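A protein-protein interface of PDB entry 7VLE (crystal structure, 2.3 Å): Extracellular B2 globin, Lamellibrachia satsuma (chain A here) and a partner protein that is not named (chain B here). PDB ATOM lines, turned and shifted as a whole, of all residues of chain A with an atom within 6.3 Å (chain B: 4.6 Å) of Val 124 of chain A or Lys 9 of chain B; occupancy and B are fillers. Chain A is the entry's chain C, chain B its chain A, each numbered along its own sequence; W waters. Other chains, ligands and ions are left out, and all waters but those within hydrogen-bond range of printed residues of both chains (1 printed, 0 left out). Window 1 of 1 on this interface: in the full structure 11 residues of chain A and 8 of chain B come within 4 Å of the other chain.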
ATOM      1  N   ASN A  19      19.351  28.893   1.322  1.00  0.00           N
ATOM      2  CA  ASN A  19      19.846  27.531   1.493  1.00  0.00           C
ATOM      3  C   ASN A  19      19.742  27.042   2.930  1.00  0.00           C
ATOM      4  O   ASN A  19      20.226  25.939   3.227  1.00  0.00           O
ATOM      5  CB  ASN A  19      21.293  27.442   1.006  1.00  0.00           C
ATOM      6  CG  ASN A  19      21.396  27.330  -0.506  1.00  0.00           C
ATOM      7  OD1 ASN A  19      21.040  28.255  -1.237  1.00  0.00           O
ATOM      8  ND2 ASN A  19      21.890  26.193  -0.982  1.00  0.00           N
ATOM      9  N   VAL A  20      19.135  27.828   3.822  1.00  0.00           N
ATOM     10  CA  VAL A  20      18.954  27.440   5.216  1.00  0.00           C
ATOM     11  C   VAL A  20      17.503  27.657   5.626  1.00  0.00           C
ATOM     12  O   VAL A  20      16.955  26.907   6.441  1.00  0.00           O
ATOM     13  CB  VAL A  20      19.898  28.217   6.148  1.00  0.00           C
ATOM     14  CG1 VAL A  20      19.890  27.593   7.523  1.00  0.00           C
ATOM     15  CG2 VAL A  20      21.294  28.228   5.588  1.00  0.00           C
ATOM     16  N   ARG A  28      13.406  24.837  11.270  1.00  0.00           N
ATOM     17  CA  ARG A  28      14.708  25.405  10.954  1.00  0.00           C
ATOM     18  C   ARG A  28      14.826  26.860  11.386  1.00  0.00           C
ATOM     19  O   ARG A  28      15.894  27.284  11.833  1.00  0.00           O
ATOM     20  CB  ARG A  28      14.993  25.269   9.469  1.00  0.00           C
ATOM     21  CG  ARG A  28      15.844  24.091   9.182  1.00  0.00           C
ATOM     22  CD  ARG A  28      16.472  24.247   7.867  1.00  0.00           C
ATOM     23  NE  ARG A  28      15.533  24.388   6.755  1.00  0.00           N
ATOM     24  CZ  ARG A  28      14.862  23.377   6.209  1.00  0.00           C
ATOM     25  NH1 ARG A  28      14.048  23.584   5.183  1.00  0.00           N
ATOM     26  NH2 ARG A  28      14.994  22.154   6.703  1.00  0.00           N
ATOM     27  N   ILE A  32      17.592  28.205  14.418  1.00  0.00           N
ATOM     28  CA  ILE A  32      18.576  29.256  14.164  1.00  0.00           C
ATOM     29  C   ILE A  32      18.402  30.402  15.151  1.00  0.00           C
ATOM     30  O   ILE A  32      19.370  30.890  15.748  1.00  0.00           O
ATOM     31  CB  ILE A  32      18.457  29.765  12.717  1.00  0.00           C
ATOM     32  CG1 ILE A  32      18.754  28.657  11.712  1.00  0.00           C
ATOM     33  CG2 ILE A  32      19.371  30.963  12.495  1.00  0.00           C
ATOM     34  CD1 ILE A  32      18.362  29.036  10.310  1.00  0.00           C
ATOM     35  N   VAL A 120      26.613  31.207  14.621  1.00  0.00           N
ATOM     36  CA  VAL A 120      25.528  30.264  14.357  1.00  0.00           C
ATOM     37  C   VAL A 120      25.512  29.856  12.887  1.00  0.00           C
ATOM     38  O   VAL A 120      25.427  28.667  12.557  1.00  0.00           O
ATOM     39  CB  VAL A 120      24.180  30.881  14.773  1.00  0.00           C
ATOM     40  CG1 VAL A 120      23.027  30.035  14.261  1.00  0.00           C
ATOM     41  CG2 VAL A 120      24.105  31.044  16.283  1.00  0.00           C
ATOM     42  N   MET A 121      25.590  30.840  11.989  1.00  0.00           N
ATOM     43  CA  MET A 121      25.328  30.592  10.572  1.00  0.00           C
ATOM     44  C   MET A 121      26.249  29.566   9.917  1.00  0.00           C
ATOM     45  O   MET A 121      25.738  28.731   9.151  1.00  0.00           O
ATOM     46  CB  MET A 121      25.384  31.916   9.798  1.00  0.00           C
ATOM     47  CG  MET A 121      24.200  32.834  10.040  1.00  0.00           C
ATOM     48  SD  MET A 121      22.640  32.098   9.521  1.00  0.00           S
ATOM     49  CE  MET A 121      22.963  31.814   7.782  1.00  0.00           C
ATOM     50  N   PRO A 122      27.571  29.574  10.124  1.00  0.00           N
ATOM     51  CA  PRO A 122      28.398  28.539   9.482  1.00  0.00           C
ATOM     52  C   PRO A 122      28.084  27.133   9.959  1.00  0.00           C
ATOM     53  O   PRO A 122      28.390  26.169   9.247  1.00  0.00           O
ATOM     54  CB  PRO A 122      29.831  28.950   9.850  1.00  0.00           C
ATOM     55  CG  PRO A 122      29.684  29.780  11.072  1.00  0.00           C
ATOM     56  CD  PRO A 122      28.399  30.524  10.888  1.00  0.00           C
ATOM     57  N   GLN A 123      27.473  26.985  11.138  1.00  0.00           N
ATOM     58  CA  GLN A 123      27.112  25.671  11.655  1.00  0.00           C
ATOM     59  C   GLN A 123      25.894  25.081  10.962  1.00  0.00           C
ATOM     60  O   GLN A 123      25.681  23.866  11.036  1.00  0.00           O
ATOM     61  CB  GLN A 123      26.843  25.753  13.159  1.00  0.00           C
ATOM     62  CG  GLN A 123      28.045  26.159  13.991  1.00  0.00           C
ATOM     63  CD  GLN A 123      27.694  26.360  15.452  1.00  0.00           C
ATOM     64  OE1 GLN A 123      27.023  25.528  16.064  1.00  0.00           O
ATOM     65  NE2 GLN A 123      28.140  27.474  16.018  1.00  0.00           N
ATOM     66  N   VAL A 124      25.092  25.909  10.301  1.00  0.00           N
ATOM     67  CA  VAL A 124      23.869  25.449   9.661  1.00  0.00           C
ATOM     68  C   VAL A 124      23.831  25.761   8.172  1.00  0.00           C
ATOM     69  O   VAL A 124      23.105  25.080   7.428  1.00  0.00           O
ATOM     70  CB  VAL A 124      22.630  26.045  10.366  1.00  0.00           C
ATOM     71  CG1 VAL A 124      22.478  27.524  10.028  1.00  0.00           C
ATOM     72  CG2 VAL A 124      21.371  25.258  10.027  1.00  0.00           C
ATOM     73  N   ALA A 125      24.595  26.743   7.701  1.00  0.00           N
ATOM     74  CA  ALA A 125      24.605  27.147   6.305  1.00  0.00           C
ATOM     75  C   ALA A 125      25.767  26.496   5.574  1.00  0.00           C
ATOM     76  O   ALA A 125      26.880  26.411   6.102  1.00  0.00           O
ATOM     77  CB  ALA A 125      24.708  28.668   6.176  1.00  0.00           C
ATOM     78  N   SER A 126      25.503  26.041   4.357  1.00  0.00           N
ATOM     79  CA  SER A 126      26.549  25.542   3.481  1.00  0.00           C
ATOM     80  C   SER A 126      27.072  26.681   2.616  1.00  0.00           C
ATOM     81  O   SER A 126      26.327  27.591   2.245  1.00  0.00           O
ATOM     82  CB  SER A 126      26.021  24.404   2.603  1.00  0.00           C
ATOM     83  OG  SER A 126      25.492  23.355   3.396  1.00  0.00           O
ATOM     84  N   CYS A 127      28.371  26.634   2.317  1.00  0.00           N
ATOM     85  CA  CYS A 127      29.023  27.642   1.475  1.00  0.00           C
ATOM     86  C   CYS A 127      28.919  29.038   2.082  1.00  0.00           C
ATOM     87  O   CYS A 127      28.624  30.009   1.384  1.00  0.00           O
ATOM     88  CB  CYS A 127      28.440  27.654   0.061  1.00  0.00           C
ATOM     89  SG  CYS A 127      28.264  26.069  -0.728  1.00  0.00           S
ATOM     90  N   LEU B   5      21.995  22.332  15.210  1.00  0.00           N
ATOM     91  CA  LEU B   5      22.421  22.990  13.980  1.00  0.00           C
ATOM     92  C   LEU B   5      23.069  21.994  13.029  1.00  0.00           C
ATOM     93  O   LEU B   5      22.754  21.963  11.834  1.00  0.00           O
ATOM     94  CB  LEU B   5      23.382  24.135  14.302  1.00  0.00           C
ATOM     95  CG  LEU B   5      22.799  25.261  15.155  1.00  0.00           C
ATOM     96  CD1 LEU B   5      23.766  26.433  15.237  1.00  0.00           C
ATOM     97  CD2 LEU B   5      21.454  25.700  14.597  1.00  0.00           C
ATOM     98  N   GLN B   6      23.977  21.164  13.551  1.00  0.00           N
ATOM     99  CA  GLN B   6      24.617  20.144  12.730  1.00  0.00           C
ATOM    100  C   GLN B   6      23.607  19.136  12.203  1.00  0.00           C
ATOM    101  O   GLN B   6      23.768  18.622  11.090  1.00  0.00           O
ATOM    102  CB  GLN B   6      25.708  19.440  13.538  1.00  0.00           C
ATOM    103  CG  GLN B   6      26.805  20.373  14.027  1.00  0.00           C
ATOM    104  CD  GLN B   6      27.906  19.647  14.772  1.00  0.00           C
ATOM    105  OE1 GLN B   6      27.654  18.953  15.756  1.00  0.00           O
ATOM    106  NE2 GLN B   6      29.139  19.801  14.303  1.00  0.00           N
ATOM    107  N   ARG B   7      22.560  18.842  12.981  1.00  0.00           N
ATOM    108  CA  ARG B   7      21.512  17.941  12.512  1.00  0.00           C
ATOM    109  C   ARG B   7      20.761  18.536  11.328  1.00  0.00           C
ATOM    110  O   ARG B   7      20.453  17.829  10.362  1.00  0.00           O
ATOM    111  CB  ARG B   7      20.549  17.617  13.653  1.00  0.00           C
ATOM    112  CG  ARG B   7      21.102  16.621  14.656  1.00  0.00           C
ATOM    113  CD  ARG B   7      20.339  16.631  15.970  1.00  0.00           C
ATOM    114  NE  ARG B   7      21.076  15.930  17.018  1.00  0.00           N
ATOM    115  CZ  ARG B   7      20.790  14.705  17.452  1.00  0.00           C
ATOM    116  NH1 ARG B   7      19.768  14.035  16.937  1.00  0.00           N
ATOM    117  NH2 ARG B   7      21.525  14.154  18.407  1.00  0.00           N
ATOM    118  N   LEU B   8      20.453  19.834  11.389  1.00  0.00           N
ATOM    119  CA  LEU B   8      19.823  20.506  10.257  1.00  0.00           C
ATOM    120  C   LEU B   8      20.765  20.558   9.063  1.00  0.00           C
ATOM    121  O   LEU B   8      20.361  20.290   7.926  1.00  0.00           O
ATOM    122  CB  LEU B   8      19.394  21.916  10.658  1.00  0.00           C
ATOM    123  CG  LEU B   8      18.317  22.026  11.734  1.00  0.00           C
ATOM    124  CD1 LEU B   8      17.998  23.485  12.006  1.00  0.00           C
ATOM    125  CD2 LEU B   8      17.071  21.266  11.311  1.00  0.00           C
ATOM    126  N   LYS B   9      22.027  20.920   9.310  1.00  0.00           N
ATOM    127  CA  LYS B   9      23.040  20.938   8.261  1.00  0.00           C
ATOM    128  C   LYS B   9      23.127  19.588   7.559  1.00  0.00           C
ATOM    129  O   LYS B   9      23.124  19.510   6.325  1.00  0.00           O
ATOM    130  CB  LYS B   9      24.389  21.322   8.875  1.00  0.00           C
ATOM    131  CG  LYS B   9      25.533  21.475   7.892  1.00  0.00           C
ATOM    132  CD  LYS B   9      25.377  22.733   7.063  1.00  0.00           C
ATOM    133  CE  LYS B   9      26.715  23.194   6.511  1.00  0.00           C
ATOM    134  NZ  LYS B   9      27.638  23.636   7.593  1.00  0.00           N
ATOM    135  N   VAL B  10      23.190  18.509   8.345  1.00  0.00           N
ATOM    136  CA  VAL B  10      23.258  17.160   7.787  1.00  0.00           C
ATOM    137  C   VAL B  10      22.006  16.847   6.974  1.00  0.00           C
ATOM    138  O   VAL B  10      22.085  16.243   5.898  1.00  0.00           O
ATOM    139  CB  VAL B  10      23.476  16.133   8.916  1.00  0.00           C
ATOM    140  CG1 VAL B  10      23.153  14.727   8.439  1.00  0.00           C
ATOM    141  CG2 VAL B  10      24.906  16.200   9.428  1.00  0.00           C
ATOM    142  N   LYS B  11      20.833  17.247   7.477  1.00  0.00           N
ATOM    143  CA  LYS B  11      19.591  17.009   6.742  1.00  0.00           C
ATOM    144  C   LYS B  11      19.587  17.747   5.409  1.00  0.00           C
ATOM    145  O   LYS B  11      19.136  17.207   4.392  1.00  0.00           O
ATOM    146  CB  LYS B  11      18.386  17.434   7.583  1.00  0.00           C
ATOM    147  CG  LYS B  11      18.055  16.505   8.739  1.00  0.00           C
ATOM    148  CD  LYS B  11      16.748  16.896   9.421  1.00  0.00           C
ATOM    149  CE  LYS B  11      15.550  16.657   8.513  1.00  0.00           C
ATOM    150  NZ  LYS B  11      14.259  16.816   9.241  1.00  0.00           N
ATOM    151  N   MET B  12      20.075  18.990   5.404  1.00  0.00           N
ATOM    152  CA  MET B  12      20.187  19.765   4.172  1.00  0.00           C
ATOM    153  C   MET B  12      21.057  19.051   3.149  1.00  0.00           C
ATOM    154  O   MET B  12      20.611  18.721   2.045  1.00  0.00           O
ATOM    155  CB  MET B  12      20.789  21.134   4.478  1.00  0.00           C
ATOM    156  CG  MET B  12      19.937  22.022   5.316  1.00  0.00           C
ATOM    157  SD  MET B  12      18.619  22.698   4.320  1.00  0.00           S
ATOM    158  CE  MET B  12      18.301  24.125   5.298  1.00  0.00           C
ATOM    159  N   GLN B  13      22.323  18.827   3.508  1.00  0.00           N
ATOM    160  CA  GLN B  13      23.289  18.273   2.568  1.00  0.00           C
ATOM    161  C   GLN B  13      22.922  16.856   2.153  1.00  0.00           C
ATOM    162  O   GLN B  13      23.243  16.436   1.035  1.00  0.00           O
ATOM    163  CB  GLN B  13      24.684  18.312   3.185  1.00  0.00           C
ATOM    164  CG  GLN B  13      25.118  19.703   3.629  1.00  0.00           C
ATOM    165  CD  GLN B  13      26.569  19.755   4.062  1.00  0.00           C
ATOM    166  OE1 GLN B  13      27.182  18.725   4.340  1.00  0.00           O
ATOM    167  NE2 GLN B  13      27.128  20.958   4.115  1.00  0.00           N
ATOM    168  N   ASP B 124      30.105  19.595   4.982  1.00  0.00           N
ATOM    169  CA  ASP B 124      30.517  19.808   6.371  1.00  0.00           C
ATOM    170  C   ASP B 124      30.916  18.461   6.964  1.00  0.00           C
ATOM    171  O   ASP B 124      30.121  17.784   7.617  1.00  0.00           O
ATOM    172  CB  ASP B 124      29.398  20.469   7.169  1.00  0.00           C
ATOM    173  CG  ASP B 124      29.863  20.981   8.527  1.00  0.00           C
ATOM    174  OD1 ASP B 124      30.852  20.449   9.074  1.00  0.00           O
ATOM    175  OD2 ASP B 124      29.229  21.920   9.051  1.00  0.00           O
HETATM  176  O   HOH W   1      27.845  22.251  11.002  1.00  0.00           O
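Val 20 of chain A touches Met 12 of chain B.
CG of Arg 28 of chain A touches CD1 of Leu 8 of chain B, 3.6 Å away.
Arg 28 of chain A touches Met 12 of chain B.
Leu 5 of chain B touches Val 120 of chain A (CD1 to CG1, 3.8 Å).
OE1 of Gln 123 of chain A touches CD1 of Leu 5 of chain B, 3.5 Å away.
CB of Lys 9 of chain B touches O of Gln 123 of chain A, at 3.6 Å.
Leu 8 of chain B touches Val 124 of chain A.
Val 124 of chain A touches Lys 9 of chain B (O to CD, 3.3 Å).
Lys 9 of chain B touches Ser 126 of chain A.
Water W1 lies within hydrogen-bond range of OD2 of Asp 124 of chain B (2.4 Å) and O of Gln 123 of chain A (2.7 Å).
NZ of Lys 9 of chain B sits at hydrogen-bond distance from O of Pro 122 of chain A, at 3.1 Å.
NZ of Lys 9 of chain B lies within hydrogen-bond range of O of Ala 125 of chain A (3.2 Å).
OG of Ser 126 of chain A sits at hydrogen-bond distance from NE2 of Gln 13 of chain B, at 3.0 Å.
The backbone carbonyl oxygen of Asn 19 of chain A lies close to the side-chain sulfur of Met 12 of chain B, at 3.8 Å.
Of the printed residues of chain B, Asn 19 of chain A touches Met 12 (3.4 Å).
Of the printed residues of chain B, Val 124 of chain A touches Leu 8 and Lys 9.
Of the printed residues of chain B, Ser 126 of chain A touches Lys 9 (3.4 Å) and Gln 13 (3.0 Å).
Of the printed residues of chain A, Leu 5 of chain B touches Val 120 and Gln 123.
Gln 6 of chain B touches none of the printed residues of chain A.
Printed residues of chain A within 4 Å of Leu 8 of chain B: Arg 28 (3.6 Å) and Val 124 (3.9 Å).
Printed residues of chain A within 4 Å of Lys 9 of chain B: Pro 122, Gln 123, Val 124, Ala 125 and Ser 126.
Lys 11 of chain B touches none of the printed residues of chain A.
Printed residues of chain A within 4 Å of Gln 13 of chain B: Ser 126.
The side-chain amino group of Lys 9 of chain B lies within salt-bridge range of the side-chain carboxylate of Asp 124 of chain B.
OE1 of Gln 13 of chain B sits at hydrogen-bond distance from N of Asp 124 of chain B (3.1 Å).
O of Val 20 of chain A sits at hydrogen-bond distance from NE of Arg 28 of chain A, 2.9 Å away.
Of the 12 printed residues of chain A, 9 touch a printed residue of chain B.
Printed residues of chain A that touch a printed residue of chain B: Asn 19, Val 20, Arg 28, Val 120, Pro 122, Gln 123, Val 124, Ala 125 and Ser 126.
Hydrophobic or aromatic side chains of chain A that line the printed part of chain B: Val 120 and Val 124.
Of the 10 printed residues of chain B, 5 touch a printed residue of chain A.
Hydrophobic or aromatic side chains of chain B within 4 Å of the printed part of chain A: Leu 5, Leu 8 and Met 12.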
